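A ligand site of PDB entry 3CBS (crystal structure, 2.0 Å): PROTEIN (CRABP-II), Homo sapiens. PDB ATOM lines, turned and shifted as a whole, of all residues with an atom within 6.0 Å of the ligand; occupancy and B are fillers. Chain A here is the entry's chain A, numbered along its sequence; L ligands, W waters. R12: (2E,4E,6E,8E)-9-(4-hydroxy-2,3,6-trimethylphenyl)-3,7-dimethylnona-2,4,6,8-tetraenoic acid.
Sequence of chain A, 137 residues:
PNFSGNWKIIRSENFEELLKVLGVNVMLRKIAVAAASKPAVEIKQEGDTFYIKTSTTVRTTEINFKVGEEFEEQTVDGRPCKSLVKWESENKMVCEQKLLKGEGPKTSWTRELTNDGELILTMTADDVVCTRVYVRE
Merely in contact with the ligand: Leu 19, Leu 28, Ala 32, Ala 36, Pro 39, Thr 54, Thr 56, Val 58, Arg 59, Val 76 and Leu 121. Hydrophobic or aromatic side chains within 4 Å of the ligand: Leu 19, Leu 28, Ala 32, Ala 36, Pro 39, Val 58, Leu 121 and Tyr 134. Within 4 Å of the ligand: Leu 19, Leu 28, Ala 32, Ala 36, Pro 39, Thr 54, Thr 56, Val 58, Arg 59, Val 76, Leu 121, Arg 132 and Tyr 134. The nearest printed residue that does not touch the ligand is Ala 35 (4.03 Å).
Water W1 lies within hydrogen-bond range of an oxygen (O2) of the ligand (2.7 Å), the guanidinium group (NH2) of Arg 111 (2.8 Å) and the side-chain hydroxyl (OG1) of Thr 54 (2.9 Å).
NH2 of Arg 132 sits at hydrogen-bond distance from O of Ala 36 (2.8 Å). O of Arg 59 is in hydrogen-bond range of OG1 of Thr 56 (2.6 Å). N of Leu 121 lies within hydrogen-bond range of O of Arg 132 (2.7 Å). The backbone NH (N) of Val 24 lies within hydrogen-bond range of the backbone carbonyl oxygen (O) of Leu 19 (3.2 Å). The backbone NH (N) of Val 58 sits close to the side-chain hydroxyl (OG1) of Thr 56 (3.5 Å). OH of Tyr 134 is in hydrogen-bond range of NE of Arg 132 (3.1 Å).
NH2 of Arg 132 is in salt-bridge range of O3 of the ligand, at 2.7 Å. The side-chain hydroxyl of Tyr 134 is in hydrogen-bond range of an oxygen (O3) of the ligand.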
ATOM      1  N   ILE A   9      -6.752   8.170  -9.212  1.00  0.00           N
ATOM      2  CA  ILE A   9      -5.726   7.180  -8.977  1.00  0.00           C
ATOM      3  C   ILE A   9      -6.171   6.121  -7.962  1.00  0.00           C
ATOM      4  O   ILE A   9      -6.888   6.424  -7.013  1.00  0.00           O
ATOM      5  CB  ILE A   9      -4.425   7.852  -8.494  1.00  0.00           C
ATOM      6  CG1 ILE A   9      -3.269   6.857  -8.583  1.00  0.00           C
ATOM      7  CG2 ILE A   9      -4.601   8.368  -7.066  1.00  0.00           C
ATOM      8  CD1 ILE A   9      -1.899   7.477  -8.361  1.00  0.00           C
ATOM      9  N   PHE A  15       6.744   5.888  -6.472  1.00  0.00           N
ATOM     10  CA  PHE A  15       6.750   7.310  -6.787  1.00  0.00           C
ATOM     11  C   PHE A  15       7.839   8.013  -5.968  1.00  0.00           C
ATOM     12  O   PHE A  15       8.554   8.863  -6.475  1.00  0.00           O
ATOM     13  CB  PHE A  15       5.383   7.920  -6.505  1.00  0.00           C
ATOM     14  CG  PHE A  15       5.286   9.374  -6.886  1.00  0.00           C
ATOM     15  CD1 PHE A  15       5.454   9.768  -8.211  1.00  0.00           C
ATOM     16  CD2 PHE A  15       5.023  10.343  -5.928  1.00  0.00           C
ATOM     17  CE1 PHE A  15       5.366  11.108  -8.563  1.00  0.00           C
ATOM     18  CE2 PHE A  15       4.936  11.683  -6.279  1.00  0.00           C
ATOM     19  CZ  PHE A  15       5.108  12.066  -7.597  1.00  0.00           C
ATOM     20  N   LEU A  19      11.278  10.057  -7.297  1.00  0.00           N
ATOM     21  CA  LEU A  19      11.680  11.401  -6.910  1.00  0.00           C
ATOM     22  C   LEU A  19      13.089  11.395  -6.311  1.00  0.00           C
ATOM     23  O   LEU A  19      13.869  12.298  -6.562  1.00  0.00           O
ATOM     24  CB  LEU A  19      10.684  11.996  -5.917  1.00  0.00           C
ATOM     25  CG  LEU A  19       9.230  12.050  -6.417  1.00  0.00           C
ATOM     26  CD1 LEU A  19       8.370  12.752  -5.374  1.00  0.00           C
ATOM     27  CD2 LEU A  19       9.157  12.795  -7.738  1.00  0.00           C
ATOM     28  N   VAL A  24      15.049  15.127  -5.602  1.00  0.00           N
ATOM     29  CA  VAL A  24      14.087  15.859  -4.786  1.00  0.00           C
ATOM     30  C   VAL A  24      14.423  15.617  -3.311  1.00  0.00           C
ATOM     31  O   VAL A  24      14.529  14.462  -2.883  1.00  0.00           O
ATOM     32  CB  VAL A  24      12.651  15.369  -5.097  1.00  0.00           C
ATOM     33  CG1 VAL A  24      11.636  16.156  -4.281  1.00  0.00           C
ATOM     34  CG2 VAL A  24      12.369  15.507  -6.589  1.00  0.00           C
ATOM     35  N   LEU A  28      10.479  17.508   0.537  1.00  0.00           N
ATOM     36  CA  LEU A  28       9.681  17.774  -0.660  1.00  0.00           C
ATOM     37  C   LEU A  28       9.101  16.460  -1.142  1.00  0.00           C
ATOM     38  O   LEU A  28       7.991  16.396  -1.671  1.00  0.00           O
ATOM     39  CB  LEU A  28      10.542  18.361  -1.765  1.00  0.00           C
ATOM     40  CG  LEU A  28      10.362  19.830  -2.110  1.00  0.00           C
ATOM     41  CD1 LEU A  28      11.230  20.160  -3.323  1.00  0.00           C
ATOM     42  CD2 LEU A  28       8.904  20.116  -2.415  1.00  0.00           C
ATOM     43  N   ILE A  31       6.074  15.726   0.842  1.00  0.00           N
ATOM     44  CA  ILE A  31       5.035  16.656   0.425  1.00  0.00           C
ATOM     45  C   ILE A  31       4.475  16.227  -0.934  1.00  0.00           C
ATOM     46  O   ILE A  31       3.259  16.187  -1.140  1.00  0.00           O
ATOM     47  CB  ILE A  31       5.594  18.093   0.300  1.00  0.00           C
ATOM     48  CG1 ILE A  31       6.083  18.587   1.670  1.00  0.00           C
ATOM     49  CG2 ILE A  31       4.526  19.023  -0.273  1.00  0.00           C
ATOM     50  CD1 ILE A  31       6.789  19.918   1.614  1.00  0.00           C
ATOM     51  N   ALA A  32       5.374  15.898  -1.860  1.00  0.00           N
ATOM     52  CA  ALA A  32       4.995  15.474  -3.204  1.00  0.00           C
ATOM     53  C   ALA A  32       4.153  14.206  -3.193  1.00  0.00           C
ATOM     54  O   ALA A  32       3.110  14.143  -3.828  1.00  0.00           O
ATOM     55  CB  ALA A  32       6.243  15.252  -4.048  1.00  0.00           C
ATOM     56  N   VAL A  33       4.624  13.197  -2.472  1.00  0.00           N
ATOM     57  CA  VAL A  33       3.911  11.925  -2.372  1.00  0.00           C
ATOM     58  C   VAL A  33       2.492  12.157  -1.857  1.00  0.00           C
ATOM     59  O   VAL A  33       1.535  11.610  -2.413  1.00  0.00           O
ATOM     60  CB  VAL A  33       4.651  10.953  -1.417  1.00  0.00           C
ATOM     61  CG1 VAL A  33       3.809   9.723  -1.163  1.00  0.00           C
ATOM     62  CG2 VAL A  33       5.971  10.553  -2.032  1.00  0.00           C
ATOM     63  N   ALA A  35       0.662  15.001  -1.886  1.00  0.00           N
ATOM     64  CA  ALA A  35      -0.112  15.727  -2.880  1.00  0.00           C
ATOM     65  C   ALA A  35      -0.482  14.832  -4.056  1.00  0.00           C
ATOM     66  O   ALA A  35      -1.604  14.888  -4.556  1.00  0.00           O
ATOM     67  CB  ALA A  35       0.686  16.932  -3.376  1.00  0.00           C
ATOM     68  N   ALA A  36       0.466  14.012  -4.495  1.00  0.00           N
ATOM     69  CA  ALA A  36       0.270  13.120  -5.628  1.00  0.00           C
ATOM     70  C   ALA A  36      -0.578  11.899  -5.323  1.00  0.00           C
ATOM     71  O   ALA A  36      -0.861  11.103  -6.228  1.00  0.00           O
ATOM     72  CB  ALA A  36       1.621  12.685  -6.183  1.00  0.00           C
ATOM     73  N   PRO A  39      -4.470  13.211  -6.896  1.00  0.00           N
ATOM     74  CA  PRO A  39      -4.488  14.142  -8.011  1.00  0.00           C
ATOM     75  C   PRO A  39      -5.832  14.129  -8.739  1.00  0.00           C
ATOM     76  O   PRO A  39      -6.627  13.201  -8.574  1.00  0.00           O
ATOM     77  CB  PRO A  39      -3.370  13.612  -8.893  1.00  0.00           C
ATOM     78  CG  PRO A  39      -3.592  12.116  -8.753  1.00  0.00           C
ATOM     79  CD  PRO A  39      -3.645  12.035  -7.232  1.00  0.00           C
ATOM     80  N   VAL A  41      -7.117  14.181 -12.505  1.00  0.00           N
ATOM     81  CA  VAL A  41      -6.602  14.045 -13.854  1.00  0.00           C
ATOM     82  C   VAL A  41      -7.708  14.186 -14.871  1.00  0.00           C
ATOM     83  O   VAL A  41      -8.712  13.463 -14.834  1.00  0.00           O
ATOM     84  CB  VAL A  41      -5.911  12.691 -14.042  1.00  0.00           C
ATOM     85  CG1 VAL A  41      -5.410  12.540 -15.477  1.00  0.00           C
ATOM     86  CG2 VAL A  41      -4.746  12.577 -13.067  1.00  0.00           C
ATOM     87  N   THR A  54      -3.126  17.560 -14.951  1.00  0.00           N
ATOM     88  CA  THR A  54      -2.932  16.800 -13.721  1.00  0.00           C
ATOM     89  C   THR A  54      -2.801  17.818 -12.597  1.00  0.00           C
ATOM     90  O   THR A  54      -1.832  18.570 -12.554  1.00  0.00           O
ATOM     91  CB  THR A  54      -1.667  15.927 -13.812  1.00  0.00           C
ATOM     92  OG1 THR A  54      -1.739  15.096 -14.973  1.00  0.00           O
ATOM     93  CG2 THR A  54      -1.551  15.031 -12.564  1.00  0.00           C
ATOM     94  N   SER A  55      -3.767  17.843 -11.697  1.00  0.00           N
ATOM     95  CA  SER A  55      -3.772  18.814 -10.606  1.00  0.00           C
ATOM     96  C   SER A  55      -3.586  18.256  -9.204  1.00  0.00           C
ATOM     97  O   SER A  55      -4.181  17.242  -8.836  1.00  0.00           O
ATOM     98  CB  SER A  55      -5.070  19.615 -10.630  1.00  0.00           C
ATOM     99  OG  SER A  55      -5.240  20.283 -11.869  1.00  0.00           O
ATOM    100  N   THR A  56      -2.753  18.933  -8.430  1.00  0.00           N
ATOM    101  CA  THR A  56      -2.528  18.584  -7.041  1.00  0.00           C
ATOM    102  C   THR A  56      -2.426  19.949  -6.372  1.00  0.00           C
ATOM    103  O   THR A  56      -2.274  20.965  -7.045  1.00  0.00           O
ATOM    104  CB  THR A  56      -1.209  17.821  -6.796  1.00  0.00           C
ATOM    105  OG1 THR A  56      -0.100  18.703  -6.990  1.00  0.00           O
ATOM    106  CG2 THR A  56      -1.110  16.644  -7.741  1.00  0.00           C
ATOM    107  N   VAL A  58       0.025  21.260  -4.663  1.00  0.00           N
ATOM    108  CA  VAL A  58       1.308  21.935  -4.811  1.00  0.00           C
ATOM    109  C   VAL A  58       1.849  22.041  -6.221  1.00  0.00           C
ATOM    110  O   VAL A  58       2.821  22.756  -6.458  1.00  0.00           O
ATOM    111  CB  VAL A  58       2.402  21.269  -3.930  1.00  0.00           C
ATOM    112  CG1 VAL A  58       1.993  21.320  -2.464  1.00  0.00           C
ATOM    113  CG2 VAL A  58       2.646  19.843  -4.360  1.00  0.00           C
ATOM    114  N   ARG A  59       1.244  21.345  -7.180  1.00  0.00           N
ATOM    115  CA  ARG A  59       1.711  21.415  -8.552  1.00  0.00           C
ATOM    116  C   ARG A  59       0.659  20.917  -9.533  1.00  0.00           C
ATOM    117  O   ARG A  59       0.086  19.841  -9.366  1.00  0.00           O
ATOM    118  CB  ARG A  59       3.004  20.603  -8.721  1.00  0.00           C
ATOM    119  CG  ARG A  59       3.556  20.519 -10.155  1.00  0.00           C
ATOM    120  CD  ARG A  59       4.857  19.718 -10.144  1.00  0.00           C
ATOM    121  NE  ARG A  59       5.353  19.331 -11.461  1.00  0.00           N
ATOM    122  CZ  ARG A  59       5.848  20.169 -12.364  1.00  0.00           C
ATOM    123  NH1 ARG A  59       5.927  21.466 -12.124  1.00  0.00           N
ATOM    124  NH2 ARG A  59       6.271  19.690 -13.535  1.00  0.00           N
ATOM    125  N   VAL A  76       8.892  15.284 -13.928  1.00  0.00           N
ATOM    126  CA  VAL A  76       8.065  15.313 -12.738  1.00  0.00           C
ATOM    127  C   VAL A  76       8.600  16.250 -11.661  1.00  0.00           C
ATOM    128  O   VAL A  76       7.819  16.778 -10.872  1.00  0.00           O
ATOM    129  CB  VAL A  76       7.895  13.882 -12.162  1.00  0.00           C
ATOM    130  CG1 VAL A  76       9.251  13.256 -11.925  1.00  0.00           C
ATOM    131  CG2 VAL A  76       7.095  13.925 -10.883  1.00  0.00           C
ATOM    132  N   ASP A  77       9.909  16.493 -11.636  1.00  0.00           N
ATOM    133  CA  ASP A  77      10.456  17.382 -10.615  1.00  0.00           C
ATOM    134  C   ASP A  77      10.610  18.829 -11.078  1.00  0.00           C
ATOM    135  O   ASP A  77      11.321  19.633 -10.453  1.00  0.00           O
ATOM    136  CB  ASP A  77      11.795  16.833 -10.087  1.00  0.00           C
ATOM    137  CG  ASP A  77      12.909  16.883 -11.118  1.00  0.00           C
ATOM    138  OD1 ASP A  77      12.727  16.320 -12.216  1.00  0.00           O
ATOM    139  OD2 ASP A  77      13.957  17.475 -10.813  1.00  0.00           O
ATOM    140  N   GLY A  78       9.947  19.159 -12.182  1.00  0.00           N
ATOM    141  CA  GLY A  78       9.964  20.529 -12.679  1.00  0.00           C
ATOM    142  C   GLY A  78      11.055  20.988 -13.625  1.00  0.00           C
ATOM    143  O   GLY A  78      11.230  22.198 -13.801  1.00  0.00           O
ATOM    144  N   ARG A 111       1.600   6.006 -21.141  1.00  0.00           N
ATOM    145  CA  ARG A 111       0.220   5.967 -20.696  1.00  0.00           C
ATOM    146  C   ARG A 111      -0.451   4.900 -21.551  1.00  0.00           C
ATOM    147  O   ARG A 111      -0.349   4.922 -22.773  1.00  0.00           O
ATOM    148  CB  ARG A 111      -0.475   7.320 -20.884  1.00  0.00           C
ATOM    149  CG  ARG A 111      -0.055   8.369 -19.859  1.00  0.00           C
ATOM    150  CD  ARG A 111      -0.999   9.554 -19.903  1.00  0.00           C
ATOM    151  NE  ARG A 111      -0.866  10.420 -18.737  1.00  0.00           N
ATOM    152  CZ  ARG A 111       0.140  11.261 -18.534  1.00  0.00           C
ATOM    153  NH1 ARG A 111       1.125  11.375 -19.432  1.00  0.00           N
ATOM    154  NH2 ARG A 111       0.162  12.008 -17.434  1.00  0.00           N
ATOM    155  N   LEU A 121      -0.167   4.687 -15.922  1.00  0.00           N
ATOM    156  CA  LEU A 121       0.842   5.691 -16.163  1.00  0.00           C
ATOM    157  C   LEU A 121       2.138   5.116 -15.648  1.00  0.00           C
ATOM    158  O   LEU A 121       2.216   4.681 -14.495  1.00  0.00           O
ATOM    159  CB  LEU A 121       0.547   6.983 -15.397  1.00  0.00           C
ATOM    160  CG  LEU A 121       1.717   7.978 -15.327  1.00  0.00           C
ATOM    161  CD1 LEU A 121       2.116   8.436 -16.717  1.00  0.00           C
ATOM    162  CD2 LEU A 121       1.321   9.182 -14.446  1.00  0.00           C
ATOM    163  N   MET A 123       6.193   6.024 -15.156  1.00  0.00           N
ATOM    164  CA  MET A 123       7.199   7.069 -15.221  1.00  0.00           C
ATOM    165  C   MET A 123       8.511   6.420 -14.835  1.00  0.00           C
ATOM    166  O   MET A 123       8.566   5.606 -13.913  1.00  0.00           O
ATOM    167  CB  MET A 123       6.884   8.222 -14.251  1.00  0.00           C
ATOM    168  CG  MET A 123       5.736   9.113 -14.715  1.00  0.00           C
ATOM    169  SD  MET A 123       5.423  10.469 -13.578  1.00  0.00           S
ATOM    170  CE  MET A 123       4.832   9.574 -12.182  1.00  0.00           C
ATOM    171  N   ARG A 132       1.586   3.978 -11.846  1.00  0.00           N
ATOM    172  CA  ARG A 132       0.384   4.580 -11.265  1.00  0.00           C
ATOM    173  C   ARG A 132      -0.818   4.148 -12.088  1.00  0.00           C
ATOM    174  O   ARG A 132      -0.798   4.207 -13.318  1.00  0.00           O
ATOM    175  CB  ARG A 132       0.548   6.102 -11.222  1.00  0.00           C
ATOM    176  CG  ARG A 132       1.627   6.536 -10.228  1.00  0.00           C
ATOM    177  CD  ARG A 132       2.089   7.975 -10.426  1.00  0.00           C
ATOM    178  NE  ARG A 132       1.107   9.005 -10.131  1.00  0.00           N
ATOM    179  CZ  ARG A 132       0.728   9.398  -8.913  1.00  0.00           C
ATOM    180  NH1 ARG A 132       1.242   8.840  -7.828  1.00  0.00           N
ATOM    181  NH2 ARG A 132      -0.135  10.387  -8.791  1.00  0.00           N
ATOM    182  N   TYR A 134      -5.004   4.408 -12.809  1.00  0.00           N
ATOM    183  CA  TYR A 134      -6.183   5.240 -12.643  1.00  0.00           C
ATOM    184  C   TYR A 134      -7.416   4.577 -13.230  1.00  0.00           C
ATOM    185  O   TYR A 134      -7.322   3.781 -14.159  1.00  0.00           O
ATOM    186  CB  TYR A 134      -6.006   6.586 -13.345  1.00  0.00           C
ATOM    187  CG  TYR A 134      -4.723   7.309 -13.042  1.00  0.00           C
ATOM    188  CD1 TYR A 134      -3.512   6.789 -13.471  1.00  0.00           C
ATOM    189  CD2 TYR A 134      -4.708   8.508 -12.330  1.00  0.00           C
ATOM    190  CE1 TYR A 134      -2.318   7.432 -13.219  1.00  0.00           C
ATOM    191  CE2 TYR A 134      -3.517   9.171 -12.063  1.00  0.00           C
ATOM    192  CZ  TYR A 134      -2.323   8.623 -12.519  1.00  0.00           C
ATOM    193  OH  TYR A 134      -1.128   9.226 -12.283  1.00  0.00           O
HETATM  194  C1  R12 L   1       9.726  20.114  -6.566  1.00  0.00           C
HETATM  195  C2  R12 L   1       9.668  18.762  -6.765  1.00  0.00           C
HETATM  196  C3  R12 L   1       8.436  18.091  -6.793  1.00  0.00           C
HETATM  197  C4  R12 L   1       7.251  18.833  -6.609  1.00  0.00           C
HETATM  198  C5  R12 L   1       7.305  20.235  -6.403  1.00  0.00           C
HETATM  199  C6  R12 L   1       8.566  20.883  -6.381  1.00  0.00           C
HETATM  200  C7  R12 L   1       5.929  18.149  -6.634  1.00  0.00           C
HETATM  201  C8  R12 L   1       5.435  17.395  -7.614  1.00  0.00           C
HETATM  202  C9  R12 L   1       4.198  16.704  -7.630  1.00  0.00           C
HETATM  203  C10 R12 L   1       4.001  15.856  -8.644  1.00  0.00           C
HETATM  204  C11 R12 L   1       2.797  15.167  -8.952  1.00  0.00           C
HETATM  205  C12 R12 L   1       2.703  14.332  -9.987  1.00  0.00           C
HETATM  206  C13 R12 L   1       1.543  13.623 -10.379  1.00  0.00           C
HETATM  207  C14 R12 L   1       1.613  12.770 -11.529  1.00  0.00           C
HETATM  208  C15 R12 L   1       0.613  11.940 -12.157  1.00  0.00           C
HETATM  209  C18 R12 L   1       0.271  13.760  -9.610  1.00  0.00           C
HETATM  210  C19 R12 L   1       3.173  16.945  -6.551  1.00  0.00           C
HETATM  211  C20 R12 L   1       6.033  21.023  -6.213  1.00  0.00           C
HETATM  212  C23 R12 L   1       8.451  16.594  -7.012  1.00  0.00           C
HETATM  213  O1  R12 L   1      10.909  20.788  -6.522  1.00  0.00           O
HETATM  214  O2  R12 L   1       0.522  11.856 -13.364  1.00  0.00           O
HETATM  215  O3  R12 L   1      -0.190  11.292 -11.331  1.00  0.00           O
HETATM  216  O   HOH W   1      -1.444  12.196 -15.125  1.00  0.00           O
HETATM  217  O   HOH W   2      13.169  19.379  -6.375  1.00  0.00           O
HETATM  218  O   HOH W   3       1.915  13.840 -14.742  1.00  0.00           O
